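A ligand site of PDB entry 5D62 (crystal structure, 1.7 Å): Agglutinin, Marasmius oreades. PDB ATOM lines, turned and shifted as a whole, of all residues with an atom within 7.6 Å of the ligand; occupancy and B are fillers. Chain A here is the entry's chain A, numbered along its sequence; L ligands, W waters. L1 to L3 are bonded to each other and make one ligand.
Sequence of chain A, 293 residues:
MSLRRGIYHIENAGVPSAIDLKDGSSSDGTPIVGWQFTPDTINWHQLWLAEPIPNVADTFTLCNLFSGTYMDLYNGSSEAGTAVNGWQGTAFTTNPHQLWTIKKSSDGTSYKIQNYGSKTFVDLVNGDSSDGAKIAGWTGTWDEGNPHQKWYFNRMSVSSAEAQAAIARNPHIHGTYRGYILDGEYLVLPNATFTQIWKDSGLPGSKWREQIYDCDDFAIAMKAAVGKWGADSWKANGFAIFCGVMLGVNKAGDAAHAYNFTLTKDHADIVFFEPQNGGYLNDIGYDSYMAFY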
ATOM      1  N   ASP A  28     -32.078  12.416   5.007  1.00  0.00           N
ATOM      2  CA  ASP A  28     -30.949  12.621   4.073  1.00  0.00           C
ATOM      3  C   ASP A  28     -29.980  13.596   4.684  1.00  0.00           C
ATOM      4  O   ASP A  28     -30.371  14.622   5.272  1.00  0.00           O
ATOM      5  CB  ASP A  28     -31.431  13.139   2.683  1.00  0.00           C
ATOM      6  CG  ASP A  28     -32.195  12.127   1.887  1.00  0.00           C
ATOM      7  OD1 ASP A  28     -32.089  10.879   2.097  1.00  0.00           O
ATOM      8  OD2 ASP A  28     -32.875  12.568   0.908  1.00  0.00           O
ATOM      9  N   GLY A  29     -28.717  13.305   4.666  1.00  0.00           N
ATOM     10  CA  GLY A  29     -27.674  14.158   5.164  1.00  0.00           C
ATOM     11  C   GLY A  29     -27.350  13.923   6.631  1.00  0.00           C
ATOM     12  O   GLY A  29     -26.539  14.631   7.153  1.00  0.00           O
ATOM     13  N   MET A  71     -24.623   4.828   2.796  1.00  0.00           N
ATOM     14  CA  MET A  71     -23.413   5.608   2.911  1.00  0.00           C
ATOM     15  C   MET A  71     -23.131   6.368   1.643  1.00  0.00           C
ATOM     16  O   MET A  71     -23.039   5.785   0.543  1.00  0.00           O
ATOM     17  CB  MET A  71     -22.205   4.742   3.333  1.00  0.00           C
ATOM     18  CG  MET A  71     -20.939   5.592   3.625  1.00  0.00           C
ATOM     19  SD  MET A  71     -19.492   4.539   3.924  1.00  0.00           S
ATOM     20  CE  MET A  71     -19.929   3.888   5.465  1.00  0.00           C
ATOM     21  N   ASP A  72     -23.043   7.703   1.775  1.00  0.00           N
ATOM     22  CA  ASP A  72     -23.084   8.685   0.674  1.00  0.00           C
ATOM     23  C   ASP A  72     -22.005   9.761   0.846  1.00  0.00           C
ATOM     24  O   ASP A  72     -21.927  10.439   1.872  1.00  0.00           O
ATOM     25  CB  ASP A  72     -24.511   9.291   0.592  1.00  0.00           C
ATOM     26  CG  ASP A  72     -24.673  10.252  -0.553  1.00  0.00           C
ATOM     27  OD1 ASP A  72     -24.023  11.272  -0.513  1.00  0.00           O
ATOM     28  OD2 ASP A  72     -25.458   9.972  -1.530  1.00  0.00           O
ATOM     29  N   LEU A  73     -21.137   9.915  -0.134  1.00  0.00           N
ATOM     30  CA  LEU A  73     -20.133  10.984  -0.112  1.00  0.00           C
ATOM     31  C   LEU A  73     -20.755  12.223  -0.700  1.00  0.00           C
ATOM     32  O   LEU A  73     -21.174  12.200  -1.873  1.00  0.00           O
ATOM     33  CB  LEU A  73     -18.932  10.576  -0.973  1.00  0.00           C
ATOM     34  CG  LEU A  73     -17.763  11.577  -0.996  1.00  0.00           C
ATOM     35  CD1 LEU A  73     -17.061  11.658   0.372  1.00  0.00           C
ATOM     36  CD2 LEU A  73     -16.721  11.152  -2.020  1.00  0.00           C
ATOM     37  N   TYR A  74     -20.793  13.301   0.067  1.00  0.00           N
ATOM     38  CA  TYR A  74     -21.616  14.458  -0.204  1.00  0.00           C
ATOM     39  C   TYR A  74     -21.192  15.111  -1.535  1.00  0.00           C
ATOM     40  O   TYR A  74     -20.080  15.612  -1.687  1.00  0.00           O
ATOM     41  CB  TYR A  74     -21.641  15.454   0.987  1.00  0.00           C
ATOM     42  CG  TYR A  74     -22.612  16.610   0.825  1.00  0.00           C
ATOM     43  CD1 TYR A  74     -23.952  16.382   0.810  1.00  0.00           C
ATOM     44  CD2 TYR A  74     -22.161  17.897   0.609  1.00  0.00           C
ATOM     45  CE1 TYR A  74     -24.877  17.443   0.610  1.00  0.00           C
ATOM     46  CE2 TYR A  74     -23.046  18.942   0.405  1.00  0.00           C
ATOM     47  CZ  TYR A  74     -24.422  18.673   0.387  1.00  0.00           C
ATOM     48  OH  TYR A  74     -25.374  19.671   0.205  1.00  0.00           O
ATOM     49  N   ASN A  75     -22.140  15.102  -2.461  1.00  0.00           N
ATOM     50  CA  ASN A  75     -21.966  15.587  -3.846  1.00  0.00           C
ATOM     51  C   ASN A  75     -20.825  14.960  -4.571  1.00  0.00           C
ATOM     52  O   ASN A  75     -20.368  15.461  -5.633  1.00  0.00           O
ATOM     53  CB  ASN A  75     -21.845  17.102  -3.830  1.00  0.00           C
ATOM     54  CG  ASN A  75     -23.184  17.785  -3.761  1.00  0.00           C
ATOM     55  OD1 ASN A  75     -24.179  17.281  -4.265  1.00  0.00           O
ATOM     56  ND2 ASN A  75     -23.228  18.943  -3.146  1.00  0.00           N
ATOM     57  N   GLY A  76     -20.374  13.790  -4.086  1.00  0.00           N
ATOM     58  CA  GLY A  76     -19.250  13.115  -4.707  1.00  0.00           C
ATOM     59  C   GLY A  76     -17.895  13.863  -4.752  1.00  0.00           C
ATOM     60  O   GLY A  76     -16.978  13.484  -5.520  1.00  0.00           O
ATOM     61  N   SER A  77     -17.705  14.870  -3.917  1.00  0.00           N
ATOM     62  CA  SER A  77     -16.526  15.741  -4.011  1.00  0.00           C
ATOM     63  C   SER A  77     -15.288  14.911  -3.622  1.00  0.00           C
ATOM     64  O   SER A  77     -15.288  14.190  -2.581  1.00  0.00           O
ATOM     65  CB  SER A  77     -16.675  16.966  -3.099  1.00  0.00           C
ATOM     66  OG  SER A  77     -15.474  17.743  -3.190  1.00  0.00           O
ATOM     67  N   ALA A  83     -17.990  15.593   3.639  1.00  0.00           N
ATOM     68  CA  ALA A  83     -18.881  14.784   4.539  1.00  0.00           C
ATOM     69  C   ALA A  83     -19.349  13.461   4.003  1.00  0.00           C
ATOM     70  O   ALA A  83     -19.565  13.292   2.793  1.00  0.00           O
ATOM     71  CB  ALA A  83     -20.162  15.593   4.883  1.00  0.00           C
ATOM     72  N   ASN A  85     -22.302  10.858   4.800  1.00  0.00           N
ATOM     73  CA  ASN A  85     -23.594  10.852   5.411  1.00  0.00           C
ATOM     74  C   ASN A  85     -24.469   9.687   4.911  1.00  0.00           C
ATOM     75  O   ASN A  85     -24.217   9.086   3.864  1.00  0.00           O
ATOM     76  CB  ASN A  85     -24.410  12.143   5.096  1.00  0.00           C
ATOM     77  CG  ASN A  85     -23.712  13.436   5.353  1.00  0.00           C
ATOM     78  OD1 ASN A  85     -23.333  13.740   6.478  1.00  0.00           O
ATOM     79  ND2 ASN A  85     -23.707  14.311   4.314  1.00  0.00           N
ATOM     80  N   GLY A  86     -25.528   9.425   5.664  1.00  0.00           N
ATOM     81  CA  GLY A  86     -26.620   8.593   5.257  1.00  0.00           C
ATOM     82  C   GLY A  86     -27.528   9.357   4.298  1.00  0.00           C
ATOM     83  O   GLY A  86     -27.845  10.508   4.501  1.00  0.00           O
ATOM     84  N   TRP A  87     -27.950   8.656   3.280  1.00  0.00           N
ATOM     85  CA  TRP A  87     -28.751   9.231   2.177  1.00  0.00           C
ATOM     86  C   TRP A  87     -29.644   8.195   1.519  1.00  0.00           C
ATOM     87  O   TRP A  87     -29.215   7.036   1.336  1.00  0.00           O
ATOM     88  CB  TRP A  87     -27.858   9.860   1.157  1.00  0.00           C
ATOM     89  CG  TRP A  87     -28.539  11.080   0.410  1.00  0.00           C
ATOM     90  CD1 TRP A  87     -29.490  11.032  -0.537  1.00  0.00           C
ATOM     91  CD2 TRP A  87     -28.253  12.453   0.640  1.00  0.00           C
ATOM     92  NE1 TRP A  87     -29.861  12.304  -0.937  1.00  0.00           N
ATOM     93  CE2 TRP A  87     -29.133  13.215  -0.233  1.00  0.00           C
ATOM     94  CE3 TRP A  87     -27.384  13.136   1.493  1.00  0.00           C
ATOM     95  CZ2 TRP A  87     -29.137  14.600  -0.252  1.00  0.00           C
ATOM     96  CZ3 TRP A  87     -27.412  14.598   1.474  1.00  0.00           C
ATOM     97  CH2 TRP A  87     -28.276  15.279   0.600  1.00  0.00           C
ATOM     98  N   GLN A  88     -30.864   8.634   1.113  1.00  0.00           N
ATOM     99  CA  GLN A  88     -31.734   7.678   0.367  1.00  0.00           C
ATOM    100  C   GLN A  88     -31.045   7.110  -0.873  1.00  0.00           C
ATOM    101  O   GLN A  88     -30.285   7.815  -1.550  1.00  0.00           O
ATOM    102  CB  GLN A  88     -33.108   8.248   0.037  1.00  0.00           C
ATOM    103  CG  GLN A  88     -33.077   9.438  -0.931  1.00  0.00           C
ATOM    104  CD  GLN A  88     -34.436   9.968  -1.205  1.00  0.00           C
ATOM    105  OE1 GLN A  88     -35.204   9.301  -1.839  1.00  0.00           O
ATOM    106  NE2 GLN A  88     -34.732  11.155  -0.675  1.00  0.00           N
ATOM    107  N   GLY A  89     -31.290   5.824  -1.168  1.00  0.00           N
ATOM    108  CA  GLY A  89     -30.756   5.180  -2.349  1.00  0.00           C
ATOM    109  C   GLY A  89     -31.311   3.820  -2.612  1.00  0.00           C
ATOM    110  O   GLY A  89     -32.375   3.507  -2.127  1.00  0.00           O
ATOM    111  N   THR A  90     -30.595   2.997  -3.384  1.00  0.00           N
ATOM    112  CA  THR A  90     -31.034   1.630  -3.685  1.00  0.00           C
ATOM    113  C   THR A  90     -29.797   0.742  -3.775  1.00  0.00           C
ATOM    114  O   THR A  90     -28.660   1.241  -3.967  1.00  0.00           O
ATOM    115  CB  THR A  90     -31.836   1.500  -5.015  1.00  0.00           C
ATOM    116  OG1 THR A  90     -31.024   1.907  -6.114  1.00  0.00           O
ATOM    117  CG2 THR A  90     -33.127   2.321  -4.984  1.00  0.00           C
ATOM    118  N   THR A  93     -27.627   0.878  -7.072  1.00  0.00           N
ATOM    119  CA  THR A  93     -27.580   2.199  -7.663  1.00  0.00           C
ATOM    120  C   THR A  93     -26.378   2.388  -8.574  1.00  0.00           C
ATOM    121  O   THR A  93     -25.321   1.781  -8.399  1.00  0.00           O
ATOM    122  CB  THR A  93     -27.574   3.284  -6.568  1.00  0.00           C
ATOM    123  OG1 THR A  93     -27.770   4.603  -7.125  1.00  0.00           O
ATOM    124  CG2 THR A  93     -26.291   3.228  -5.740  1.00  0.00           C
ATOM    125  N   THR A  94     -26.547   3.211  -9.608  1.00  0.00           N
ATOM    126  CA  THR A  94     -25.419   3.661 -10.400  1.00  0.00           C
ATOM    127  C   THR A  94     -24.887   5.039  -9.881  1.00  0.00           C
ATOM    128  O   THR A  94     -24.021   5.655 -10.535  1.00  0.00           O
ATOM    129  CB  THR A  94     -25.834   3.809 -11.885  1.00  0.00           C
ATOM    130  OG1 THR A  94     -26.931   4.721 -11.924  1.00  0.00           O
ATOM    131  CG2 THR A  94     -26.265   2.514 -12.517  1.00  0.00           C
ATOM    132  N   ASN A  95     -25.427   5.612  -8.794  1.00  0.00           N
ATOM    133  CA  ASN A  95     -24.955   6.927  -8.263  1.00  0.00           C
ATOM    134  C   ASN A  95     -23.601   6.689  -7.580  1.00  0.00           C
ATOM    135  O   ASN A  95     -23.558   6.019  -6.543  1.00  0.00           O
ATOM    136  CB  ASN A  95     -25.972   7.416  -7.221  1.00  0.00           C
ATOM    137  CG  ASN A  95     -25.535   8.638  -6.468  1.00  0.00           C
ATOM    138  OD1 ASN A  95     -24.427   9.147  -6.616  1.00  0.00           O
ATOM    139  ND2 ASN A  95     -26.426   9.119  -5.639  1.00  0.00           N
ATOM    140  N   PRO A  96     -22.515   7.226  -8.157  1.00  0.00           N
ATOM    141  CA  PRO A  96     -21.179   6.921  -7.586  1.00  0.00           C
ATOM    142  C   PRO A  96     -20.960   7.461  -6.168  1.00  0.00           C
ATOM    143  O   PRO A  96     -20.059   7.028  -5.456  1.00  0.00           O
ATOM    144  CB  PRO A  96     -20.218   7.565  -8.576  1.00  0.00           C
ATOM    145  CG  PRO A  96     -21.009   8.553  -9.369  1.00  0.00           C
ATOM    146  CD  PRO A  96     -22.460   8.133  -9.350  1.00  0.00           C
ATOM    147  N   HIS A  97     -21.790   8.409  -5.767  1.00  0.00           N
ATOM    148  CA  HIS A  97     -21.713   8.929  -4.390  1.00  0.00           C
ATOM    149  C   HIS A  97     -21.921   7.800  -3.354  1.00  0.00           C
ATOM    150  O   HIS A  97     -21.502   7.942  -2.186  1.00  0.00           O
ATOM    151  CB  HIS A  97     -22.740  10.030  -4.123  1.00  0.00           C
ATOM    152  CG  HIS A  97     -22.719  11.172  -5.104  1.00  0.00           C
ATOM    153  ND1 HIS A  97     -23.584  12.209  -4.994  1.00  0.00           N
ATOM    154  CD2 HIS A  97     -21.876  11.479  -6.101  1.00  0.00           C
ATOM    155  CE1 HIS A  97     -23.356  13.073  -5.979  1.00  0.00           C
ATOM    156  NE2 HIS A  97     -22.293  12.654  -6.647  1.00  0.00           N
ATOM    157  N   GLN A  98     -22.666   6.718  -3.720  1.00  0.00           N
ATOM    158  CA  GLN A  98     -23.060   5.680  -2.854  1.00  0.00           C
ATOM    159  C   GLN A  98     -22.346   4.357  -3.202  1.00  0.00           C
ATOM    160  O   GLN A  98     -22.735   3.281  -2.702  1.00  0.00           O
ATOM    161  CB  GLN A  98     -24.573   5.497  -2.915  1.00  0.00           C
ATOM    162  CG  GLN A  98     -25.271   6.703  -2.287  1.00  0.00           C
ATOM    163  CD  GLN A  98     -26.791   6.682  -2.387  1.00  0.00           C
ATOM    164  OE1 GLN A  98     -27.426   5.698  -2.779  1.00  0.00           O
ATOM    165  NE2 GLN A  98     -27.399   7.794  -1.987  1.00  0.00           N
HETATM  166  C1  LIG L   1     -29.540  10.316  -4.048  1.00  0.00           C
HETATM  167  C2  LIG L   1     -30.229   9.232  -4.794  1.00  0.00           C
HETATM  168  C3  LIG L   1     -31.194   9.821  -5.847  1.00  0.00           C
HETATM  169  C4  LIG L   1     -32.228  10.706  -5.222  1.00  0.00           C
HETATM  170  C5  LIG L   1     -31.481  11.798  -4.403  1.00  0.00           C
HETATM  171  C6  LIG L   1     -32.403  12.604  -3.543  1.00  0.00           C
HETATM  172  O1  LIG L   1     -29.211   8.401  -5.374  1.00  0.00           O
HETATM  173  O2  LIG L   1     -31.874   8.750  -6.483  1.00  0.00           O
HETATM  174  O3  LIG L   1     -33.071   9.965  -4.352  1.00  0.00           O
HETATM  175  O4  LIG L   1     -30.566  11.118  -3.470  1.00  0.00           O
HETATM  176  O5  LIG L   1     -31.669  13.684  -2.981  1.00  0.00           O
HETATM  177  C1  LG2 L   2     -26.893  14.342  -5.291  1.00  0.00           C
HETATM  178  C2  LG2 L   2     -27.516  13.030  -5.723  1.00  0.00           C
HETATM  179  C3  LG2 L   2     -28.189  12.405  -4.514  1.00  0.00           C
HETATM  180  C4  LG2 L   2     -27.158  12.274  -3.321  1.00  0.00           C
HETATM  181  C5  LG2 L   2     -26.666  13.690  -2.993  1.00  0.00           C
HETATM  182  C6  LG2 L   2     -25.627  13.833  -1.862  1.00  0.00           C
HETATM  183  O1  LG2 L   2     -27.909  15.280  -4.838  1.00  0.00           O
HETATM  184  O2  LG2 L   2     -28.457  13.192  -6.813  1.00  0.00           O
HETATM  185  O3  LG2 L   2     -28.692  11.117  -4.909  1.00  0.00           O
HETATM  186  O4  LG2 L   2     -26.098  11.320  -3.631  1.00  0.00           O
HETATM  187  O5  LG2 L   2     -26.064  14.155  -4.170  1.00  0.00           O
HETATM  188  O6  LG2 L   2     -24.366  13.240  -2.259  1.00  0.00           O
HETATM  189  C1  LG3 L   3     -28.260  12.311  -8.091  1.00  0.00           C
HETATM  190  C2  LG3 L   3     -29.513  12.615  -8.942  1.00  0.00           C
HETATM  191  C3  LG3 L   3     -29.577  14.098  -9.288  1.00  0.00           C
HETATM  192  C4  LG3 L   3     -28.301  14.476  -9.951  1.00  0.00           C
HETATM  193  C5  LG3 L   3     -27.085  14.202  -9.076  1.00  0.00           C
HETATM  194  C6  LG3 L   3     -25.775  14.425  -9.852  1.00  0.00           C
HETATM  195  O1  LG3 L   3     -30.676  12.434  -8.195  1.00  0.00           O
HETATM  196  O2  LG3 L   3     -30.593  14.236 -10.215  1.00  0.00           O
HETATM  197  O3  LG3 L   3     -28.262  13.579 -11.023  1.00  0.00           O
HETATM  198  O4  LG3 L   3     -27.077  12.853  -8.660  1.00  0.00           O
HETATM  199  O   HOH W   1     -30.609  15.390  -4.699  1.00  0.00           O
HETATM  200  O   HOH W   2     -32.908   6.429  -5.214  1.00  0.00           O
HETATM  201  O   HOH W   3     -24.797  11.292  -8.746  1.00  0.00           O
HETATM  202  O   HOH W   4     -32.900  14.607  -0.575  1.00  0.00           O
HETATM  203  O   HOH W   5     -28.918   5.792  -5.076  1.00  0.00           O
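The side-chain carboxylate (OD2) of Asp 72 is in hydrogen-bond range of an oxygen (O4) of LG2 L2 (2.6 Å).
NE1 of Trp 87 sits at hydrogen-bond distance from O4 of LIG L1 (2.9 Å).
ND2 of Asn 95 is in hydrogen-bond range of O1 of LIG L1, 2.9 Å away.
O6 of LG2 L2 is in hydrogen-bond range of N of Asn 75.
ND1 of His 97 lies within hydrogen-bond range of O4 of LG2 L2 (3.0 Å).
OE1 of Gln 88 sits at hydrogen-bond distance from O3 of LIG L1, at 3.4 Å.
The backbone carbonyl oxygen (O) of Leu 73 sits at hydrogen-bond distance from an oxygen (O6) of LG2 L2, 3.4 Å away.
The side-chain carboxylate of Asp 72 sits at hydrogen-bond distance from the side-chain amide nitrogen of Gln 98 (3.0 Å).
The side-chain amide oxygen (OD1) of Asn 95 is in hydrogen-bond range of the backbone NH (N) of His 97 (2.9 Å).
N of Asn 95 lies within hydrogen-bond range of OG1 of Thr 93 (3.0 Å).
O of His 97 lies within hydrogen-bond range of N of Leu 73 (2.9 Å).
The backbone NH (N) of Gly 76 is in hydrogen-bond range of a ring nitrogen (NE2) of His 97, 3.4 Å away.
The backbone carbonyl oxygen of Gln 88 sits at hydrogen-bond distance from the side-chain amide nitrogen of Gln 98, 2.9 Å away.
The side-chain carboxylate of Asp 28 is in hydrogen-bond range of the backbone NH of Gln 88 (2.7 Å).
The backbone NH (N) of Tyr 74 is in hydrogen-bond range of the backbone carbonyl oxygen (O) of Ala 83.
Tyr 74 touches the ligand.
Gln 98 touches the ligand.
Nine residues have an atom within 4 Å of the ligand: Asp 72, Leu 73, Tyr 74, Asn 75, Trp 87, Gln 88, Asn 95, His 97 and Gln 98.
Water W5 lies within hydrogen-bond range of the side-chain hydroxyl of Thr 93 (2.6 Å), an oxygen (O1) of LIG L1 (2.6 Å) and the side-chain amide oxygen of Gln 98 (2.7 Å).
Water W3 lies within hydrogen-bond range of O4 of LG3 L3 (2.8 Å) and OD1 of Asn 95 (3.0 Å).
Water W4 lies within hydrogen-bond range of the side-chain carboxylate (OD2) of Asp 28 (2.5 Å) and an oxygen (O5) of LIG L1 (2.9 Å).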
